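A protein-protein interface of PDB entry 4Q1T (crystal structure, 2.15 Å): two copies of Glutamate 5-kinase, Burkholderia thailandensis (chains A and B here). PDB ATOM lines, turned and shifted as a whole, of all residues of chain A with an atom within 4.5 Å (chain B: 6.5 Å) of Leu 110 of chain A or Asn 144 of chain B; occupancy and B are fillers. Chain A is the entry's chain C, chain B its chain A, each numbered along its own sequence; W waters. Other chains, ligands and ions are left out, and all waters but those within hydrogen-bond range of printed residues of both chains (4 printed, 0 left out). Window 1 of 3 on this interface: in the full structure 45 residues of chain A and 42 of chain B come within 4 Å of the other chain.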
ATOM      1  N   GLN A  88      -1.885   6.953 -19.642  1.00  0.00           N
ATOM      2  CA  GLN A  88      -2.926   6.461 -20.514  1.00  0.00           C
ATOM      3  C   GLN A  88      -2.397   6.062 -21.887  1.00  0.00           C
ATOM      4  O   GLN A  88      -2.769   5.040 -22.429  1.00  0.00           O
ATOM      5  CB  GLN A  88      -3.925   7.599 -20.729  1.00  0.00           C
ATOM      6  CG  GLN A  88      -5.184   7.276 -21.503  1.00  0.00           C
ATOM      7  CD  GLN A  88      -5.820   5.999 -21.044  1.00  0.00           C
ATOM      8  OE1 GLN A  88      -5.847   5.719 -19.849  1.00  0.00           O
ATOM      9  NE2 GLN A  88      -6.331   5.204 -21.988  1.00  0.00           N
ATOM     10  N   GLN A 108      -9.624   2.738 -27.647  1.00  0.00           N
ATOM     11  CA  GLN A 108      -9.547   3.416 -26.362  1.00  0.00           C
ATOM     12  C   GLN A 108     -10.821   4.171 -26.191  1.00  0.00           C
ATOM     13  O   GLN A 108     -11.284   4.796 -27.118  1.00  0.00           O
ATOM     14  CB  GLN A 108      -8.368   4.414 -26.311  1.00  0.00           C
ATOM     15  N   ILE A 109     -11.388   4.090 -24.997  1.00  0.00           N
ATOM     16  CA  ILE A 109     -12.608   4.767 -24.651  1.00  0.00           C
ATOM     17  C   ILE A 109     -12.384   5.398 -23.273  1.00  0.00           C
ATOM     18  O   ILE A 109     -11.789   4.785 -22.399  1.00  0.00           O
ATOM     19  CB  ILE A 109     -13.772   3.766 -24.532  1.00  0.00           C
ATOM     20  CG1 ILE A 109     -14.003   3.018 -25.854  1.00  0.00           C
ATOM     21  CG2 ILE A 109     -15.019   4.459 -24.041  1.00  0.00           C
ATOM     22  CD1 ILE A 109     -14.740   3.790 -26.910  1.00  0.00           C
ATOM     23  N   LEU A 110     -12.778   6.659 -23.113  1.00  0.00           N
ATOM     24  CA  LEU A 110     -12.695   7.335 -21.834  1.00  0.00           C
ATOM     25  C   LEU A 110     -14.099   7.760 -21.500  1.00  0.00           C
ATOM     26  O   LEU A 110     -14.770   8.385 -22.294  1.00  0.00           O
ATOM     27  CB  LEU A 110     -11.721   8.530 -21.852  1.00  0.00           C
ATOM     28  CG  LEU A 110     -10.215   8.279 -22.070  1.00  0.00           C
ATOM     29  CD1 LEU A 110      -9.433   9.569 -21.913  1.00  0.00           C
ATOM     30  CD2 LEU A 110      -9.634   7.281 -21.119  1.00  0.00           C
ATOM     31  N   LEU A 111     -14.539   7.406 -20.306  1.00  0.00           N
ATOM     32  CA  LEU A 111     -15.894   7.699 -19.847  1.00  0.00           C
ATOM     33  C   LEU A 111     -15.816   8.297 -18.450  1.00  0.00           C
ATOM     34  O   LEU A 111     -14.866   8.008 -17.718  1.00  0.00           O
ATOM     35  CB  LEU A 111     -16.700   6.381 -19.767  1.00  0.00           C
ATOM     36  CG  LEU A 111     -17.041   5.652 -21.061  1.00  0.00           C
ATOM     37  CD1 LEU A 111     -17.766   4.342 -20.757  1.00  0.00           C
ATOM     38  CD2 LEU A 111     -17.916   6.533 -21.930  1.00  0.00           C
ATOM     39  N   ASN A 142     -11.321   3.432 -19.786  1.00  0.00           N
ATOM     40  CA  ASN A 142     -10.801   4.069 -18.550  1.00  0.00           C
ATOM     41  C   ASN A 142     -11.599   5.332 -18.234  1.00  0.00           C
ATOM     42  O   ASN A 142     -12.379   5.839 -19.064  1.00  0.00           O
ATOM     43  CB  ASN A 142      -9.271   4.300 -18.592  1.00  0.00           C
ATOM     44  CG  ASN A 142      -8.630   4.519 -17.195  1.00  0.00           C
ATOM     45  OD1 ASN A 142      -9.254   4.283 -16.145  1.00  0.00           O
ATOM     46  ND2 ASN A 142      -7.362   4.967 -17.183  1.00  0.00           N
ATOM     47  N   GLU A 143     -11.436   5.780 -16.993  1.00  0.00           N
ATOM     48  CA  GLU A 143     -12.023   7.004 -16.501  1.00  0.00           C
ATOM     49  C   GLU A 143     -11.288   8.178 -17.109  1.00  0.00           C
ATOM     50  O   GLU A 143     -10.097   8.082 -17.395  1.00  0.00           O
ATOM     51  CB  GLU A 143     -11.855   7.051 -14.969  1.00  0.00           C
ATOM     52  N   ASN A 144     -12.006   9.255 -17.382  1.00  0.00           N
ATOM     53  CA  ASN A 144     -11.364  10.473 -17.888  1.00  0.00           C
ATOM     54  C   ASN A 144     -10.939  11.429 -16.754  1.00  0.00           C
ATOM     55  O   ASN A 144     -11.684  12.361 -16.414  1.00  0.00           O
ATOM     56  CB  ASN A 144     -12.290  11.184 -18.871  1.00  0.00           C
ATOM     57  CG  ASN A 144     -11.556  12.222 -19.668  1.00  0.00           C
ATOM     58  OD1 ASN A 144     -10.432  12.567 -19.324  1.00  0.00           O
ATOM     59  ND2 ASN A 144     -12.178  12.738 -20.720  1.00  0.00           N
ATOM     60  N   GLN B 108      -2.284  11.828 -23.960  1.00  0.00           N
ATOM     61  CA  GLN B 108      -3.535  11.833 -24.706  1.00  0.00           C
ATOM     62  C   GLN B 108      -4.547  12.524 -23.821  1.00  0.00           C
ATOM     63  O   GLN B 108      -4.616  12.253 -22.642  1.00  0.00           O
ATOM     64  CB  GLN B 108      -4.009  10.415 -25.080  1.00  0.00           C
ATOM     65  CG  GLN B 108      -5.263  10.357 -25.976  1.00  0.00           C
ATOM     66  CD  GLN B 108      -5.070  10.983 -27.363  1.00  0.00           C
ATOM     67  OE1 GLN B 108      -4.158  10.609 -28.099  1.00  0.00           O
ATOM     68  NE2 GLN B 108      -5.938  11.940 -27.728  1.00  0.00           N
ATOM     69  N   ILE B 109      -5.331  13.398 -24.424  1.00  0.00           N
ATOM     70  CA  ILE B 109      -6.383  14.116 -23.736  1.00  0.00           C
ATOM     71  C   ILE B 109      -7.623  14.042 -24.611  1.00  0.00           C
ATOM     72  O   ILE B 109      -7.514  14.158 -25.825  1.00  0.00           O
ATOM     73  CB  ILE B 109      -6.008  15.582 -23.552  1.00  0.00           C
ATOM     74  CG1 ILE B 109      -4.724  15.740 -22.741  1.00  0.00           C
ATOM     75  CG2 ILE B 109      -7.180  16.349 -22.956  1.00  0.00           C
ATOM     76  CD1 ILE B 109      -4.888  15.568 -21.253  1.00  0.00           C
ATOM     77  N   LEU B 110      -8.773  13.724 -24.009  1.00  0.00           N
ATOM     78  CA  LEU B 110     -10.038  13.724 -24.730  1.00  0.00           C
ATOM     79  C   LEU B 110     -10.938  14.719 -24.032  1.00  0.00           C
ATOM     80  O   LEU B 110     -11.072  14.681 -22.812  1.00  0.00           O
ATOM     81  CB  LEU B 110     -10.678  12.344 -24.790  1.00  0.00           C
ATOM     82  CG  LEU B 110      -9.977  11.219 -25.564  1.00  0.00           C
ATOM     83  CD1 LEU B 110     -10.882   9.993 -25.626  1.00  0.00           C
ATOM     84  CD2 LEU B 110      -9.635  11.586 -26.997  1.00  0.00           C
ATOM     85  N   LEU B 111     -11.482  15.649 -24.812  1.00  0.00           N
ATOM     86  CA  LEU B 111     -12.316  16.718 -24.303  1.00  0.00           C
ATOM     87  C   LEU B 111     -13.556  16.819 -25.137  1.00  0.00           C
ATOM     88  O   LEU B 111     -13.544  16.460 -26.324  1.00  0.00           O
ATOM     89  CB  LEU B 111     -11.593  18.078 -24.442  1.00  0.00           C
ATOM     90  CG  LEU B 111     -10.366  18.320 -23.592  1.00  0.00           C
ATOM     91  CD1 LEU B 111      -9.784  19.659 -23.936  1.00  0.00           C
ATOM     92  CD2 LEU B 111     -10.711  18.246 -22.138  1.00  0.00           C
ATOM     93  N   THR B 112     -14.605  17.343 -24.549  1.00  0.00           N
ATOM     94  CA  THR B 112     -15.784  17.771 -25.320  1.00  0.00           C
ATOM     95  C   THR B 112     -16.105  19.217 -24.979  1.00  0.00           C
ATOM     96  O   THR B 112     -15.812  19.656 -23.884  1.00  0.00           O
ATOM     97  CB  THR B 112     -17.039  16.933 -24.964  1.00  0.00           C
ATOM     98  OG1 THR B 112     -17.502  17.269 -23.652  1.00  0.00           O
ATOM     99  CG2 THR B 112     -16.737  15.422 -25.014  1.00  0.00           C
ATOM    100  N   ASP B 115     -17.842  19.403 -21.556  1.00  0.00           N
ATOM    101  CA  ASP B 115     -16.897  19.424 -20.425  1.00  0.00           C
ATOM    102  C   ASP B 115     -16.507  20.858 -20.098  1.00  0.00           C
ATOM    103  O   ASP B 115     -16.510  21.279 -18.948  1.00  0.00           O
ATOM    104  CB  ASP B 115     -15.602  18.653 -20.740  1.00  0.00           C
ATOM    105  CG  ASP B 115     -15.801  17.162 -20.882  1.00  0.00           C
ATOM    106  OD1 ASP B 115     -16.648  16.575 -20.166  1.00  0.00           O
ATOM    107  OD2 ASP B 115     -15.062  16.560 -21.696  1.00  0.00           O
ATOM    108  N   ASN B 142      -7.907  15.380 -28.544  1.00  0.00           N
ATOM    109  CA  ASN B 142      -8.987  15.016 -29.450  1.00  0.00           C
ATOM    110  C   ASN B 142     -10.343  15.123 -28.790  1.00  0.00           C
ATOM    111  O   ASN B 142     -10.437  15.150 -27.564  1.00  0.00           O
ATOM    112  CB  ASN B 142      -8.766  13.622 -29.943  1.00  0.00           C
ATOM    113  CG  ASN B 142      -7.565  13.559 -30.894  1.00  0.00           C
ATOM    114  OD1 ASN B 142      -6.555  12.882 -30.635  1.00  0.00           O
ATOM    115  ND2 ASN B 142      -7.676  14.286 -32.008  1.00  0.00           N
ATOM    116  N   GLU B 143     -11.384  15.183 -29.618  1.00  0.00           N
ATOM    117  CA  GLU B 143     -12.744  15.187 -29.122  1.00  0.00           C
ATOM    118  C   GLU B 143     -13.047  13.806 -28.580  1.00  0.00           C
ATOM    119  O   GLU B 143     -12.572  12.813 -29.106  1.00  0.00           O
ATOM    120  CB  GLU B 143     -13.772  15.533 -30.207  1.00  0.00           C
ATOM    121  CG  GLU B 143     -15.202  15.304 -29.723  1.00  0.00           C
ATOM    122  CD  GLU B 143     -16.269  16.005 -30.546  1.00  0.00           C
ATOM    123  OE1 GLU B 143     -16.924  15.362 -31.425  1.00  0.00           O
ATOM    124  OE2 GLU B 143     -16.482  17.202 -30.273  1.00  0.00           O
ATOM    125  N   ASN B 144     -13.875  13.743 -27.553  1.00  0.00           N
ATOM    126  CA  ASN B 144     -14.388  12.460 -27.064  1.00  0.00           C
ATOM    127  C   ASN B 144     -15.646  12.114 -27.783  1.00  0.00           C
ATOM    128  O   ASN B 144     -16.768  12.313 -27.299  1.00  0.00           O
ATOM    129  CB  ASN B 144     -14.622  12.461 -25.563  1.00  0.00           C
ATOM    130  CG  ASN B 144     -14.833  11.074 -25.044  1.00  0.00           C
ATOM    131  OD1 ASN B 144     -14.969  10.137 -25.838  1.00  0.00           O
ATOM    132  ND2 ASN B 144     -14.749  10.901 -23.739  1.00  0.00           N
ATOM    133  N   ASP B 145     -15.452  11.529 -28.957  1.00  0.00           N
ATOM    134  CA  ASP B 145     -16.532  11.206 -29.863  1.00  0.00           C
ATOM    135  C   ASP B 145     -17.423  10.082 -29.360  1.00  0.00           C
ATOM    136  O   ASP B 145     -18.471   9.837 -29.935  1.00  0.00           O
ATOM    137  CB  ASP B 145     -15.939  10.824 -31.239  1.00  0.00           C
ATOM    138  CG  ASP B 145     -15.351  12.054 -31.995  1.00  0.00           C
ATOM    139  OD1 ASP B 145     -15.941  13.164 -31.978  1.00  0.00           O
ATOM    140  OD2 ASP B 145     -14.303  11.882 -32.627  1.00  0.00           O
ATOM    141  N   THR B 146     -16.967   9.332 -28.365  1.00  0.00           N
ATOM    142  CA  THR B 146     -17.786   8.304 -27.758  1.00  0.00           C
ATOM    143  C   THR B 146     -19.031   8.908 -27.106  1.00  0.00           C
ATOM    144  O   THR B 146     -20.106   8.305 -27.139  1.00  0.00           O
ATOM    145  CB  THR B 146     -16.966   7.493 -26.742  1.00  0.00           C
ATOM    146  OG1 THR B 146     -15.859   6.858 -27.423  1.00  0.00           O
ATOM    147  CG2 THR B 146     -17.791   6.466 -26.095  1.00  0.00           C
ATOM    148  N   VAL B 147     -18.888  10.078 -26.504  1.00  0.00           N
ATOM    149  CA  VAL B 147     -19.975  10.663 -25.718  1.00  0.00           C
ATOM    150  C   VAL B 147     -20.654  11.881 -26.353  1.00  0.00           C
ATOM    151  O   VAL B 147     -21.814  12.082 -26.091  1.00  0.00           O
ATOM    152  CB  VAL B 147     -19.567  11.021 -24.276  1.00  0.00           C
ATOM    153  CG1 VAL B 147     -19.327   9.764 -23.479  1.00  0.00           C
ATOM    154  CG2 VAL B 147     -18.370  11.942 -24.228  1.00  0.00           C
ATOM    155  N   VAL B 148     -19.955  12.620 -27.217  1.00  0.00           N
ATOM    156  CA  VAL B 148     -20.522  13.786 -27.901  1.00  0.00           C
ATOM    157  C   VAL B 148     -20.165  13.755 -29.392  1.00  0.00           C
ATOM    158  O   VAL B 148     -19.010  13.637 -29.757  1.00  0.00           O
ATOM    159  CB  VAL B 148     -19.997  15.098 -27.278  1.00  0.00           C
ATOM    160  CG1 VAL B 148     -20.431  16.314 -28.090  1.00  0.00           C
ATOM    161  CG2 VAL B 148     -20.486  15.243 -25.847  1.00  0.00           C
ATOM    162  N   THR B 149     -21.181  13.836 -30.241  1.00  0.00           N
ATOM    163  CA  THR B 149     -21.015  13.653 -31.684  1.00  0.00           C
ATOM    164  C   THR B 149     -21.388  14.898 -32.509  1.00  0.00           C
ATOM    165  O   THR B 149     -21.458  14.811 -33.731  1.00  0.00           O
ATOM    166  CB  THR B 149     -21.917  12.526 -32.180  1.00  0.00           C
ATOM    167  OG1 THR B 149     -23.280  12.827 -31.859  1.00  0.00           O
ATOM    168  CG2 THR B 149     -21.529  11.201 -31.523  1.00  0.00           C
ATOM    169  N   LEU B 160     -12.420  22.551 -32.218  1.00  0.00           N
ATOM    170  CA  LEU B 160     -11.686  22.064 -31.061  1.00  0.00           C
ATOM    171  C   LEU B 160     -10.390  22.858 -30.857  1.00  0.00           C
ATOM    172  O   LEU B 160     -10.063  23.263 -29.713  1.00  0.00           O
ATOM    173  CB  LEU B 160     -11.391  20.583 -31.200  1.00  0.00           C
ATOM    174  CG  LEU B 160     -10.618  19.975 -30.016  1.00  0.00           C
ATOM    175  CD1 LEU B 160     -11.277  20.206 -28.661  1.00  0.00           C
ATOM    176  CD2 LEU B 160     -10.448  18.489 -30.272  1.00  0.00           C
HETATM  177  O   HOH W   1      -8.265  13.077 -20.979  1.00  0.00           O
HETATM  178  O   HOH W   2     -14.996  11.660 -20.795  1.00  0.00           O
HETATM  179  O   HOH W   3     -13.729   7.866 -25.702  1.00  0.00           O
HETATM  180  O   HOH W   4     -14.415  14.127 -22.458  1.00  0.00           O
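The side-chain amide nitrogen (ND2) of Asn 144 of chain A is in hydrogen-bond range of the backbone carbonyl oxygen (O) of Leu 110 of chain B. The side-chain amide nitrogen (ND2) of Asn 144 of chain B is in hydrogen-bond range of the backbone carbonyl oxygen (O) of Leu 110 of chain A (2.9 Å).
The backbone NH of Asn 144 of chain B lies within hydrogen-bond range of the backbone carbonyl oxygen of Leu 111 of chain B. The backbone NH of Thr 146 of chain B lies close to the side-chain amide oxygen of Asn 144 of chain B (3.3 Å). The backbone carbonyl oxygen of Ile 109 of chain A sits at hydrogen-bond distance from the backbone NH of Asn 142 of chain A (3.0 Å). The backbone NH (N) of Leu 111 of chain A sits at hydrogen-bond distance from the backbone carbonyl oxygen (O) of Asn 142 of chain A, at 2.9 Å. O of Leu 111 of chain A sits at hydrogen-bond distance from N of Asn 144 of chain A (3.1 Å).
Among the printed residues, merely in contact across the chains: Ile 109 of chain A with Thr 146 of chain B (3.3 Å) and Leu 111 of chain A with Val 147 of chain B (3.9 Å).
Printed residues of chain B within 4 Å of Leu 110 of chain A: Asn 144. Of the printed residues of chain B, Leu 111 of chain A touches Val 147. Thr 112 of chain B touches none of the printed residues of chain A. Glu 143 of chain B touches none of the printed residues of chain A. Of chain A, only Leu 110 (2.9 Å) comes within 4 Å of Asn 144 of chain B. Of the printed residues of chain A, Val 147 of chain B touches Leu 111 (3.9 Å). The nearest residue of chain A that does not touch Asn 144 of chain B is Asn 144 of chain A (4.4 Å). The nearest printed residue of chain B that does not touch Leu 111 of chain A is Thr 146 of chain B (4.2 Å).
Of the 15 printed residues of chain B, 4 touch a printed residue of chain A. Hydrophobic or aromatic side chains of chain B within 4 Å of the printed part of chain A: Val 147. Of the 8 printed residues of chain A, 4 touch a printed residue of chain B. Printed residues of chain A that touch a printed residue of chain B: Ile 109, Leu 110, Leu 111 and Asn 144. Among the printed residues, no Asp or Glu carboxylate lies within 4 Å of a Lys or Arg side-chain nitrogen of the other chain.
Leu 110 of chain A touches Asn 144 of chain B, and with the chains exchanged Asn 144 of chain A touches Leu 110 of chain B. 7 positions are printed for both chains. Of the 4 pairs that touch across the chains among the printed residues, 2 have their exchanged pair printed and touching as well.
Water W3 lies within hydrogen-bond range of OD1 of Asn 144 of chain B, OG1 of Thr 146 of chain B and N of Leu 110 of chain A. Water W4 lies within hydrogen-bond range of the side-chain carboxylate of Asp 115 of chain B, the side-chain amide nitrogen of Asn 144 of chain A, the backbone carbonyl oxygen of Leu 110 of chain B and the side-chain amide nitrogen of Asn 144 of chain B. Water W1 bridges OD1 of Asn 144 of chain A (2.8 Å) and N of Leu 110 of chain B (3.1 Å). Water W2 bridges ND2 of Asn 144 of chain A and ND2 of Asn 144 of chain B.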
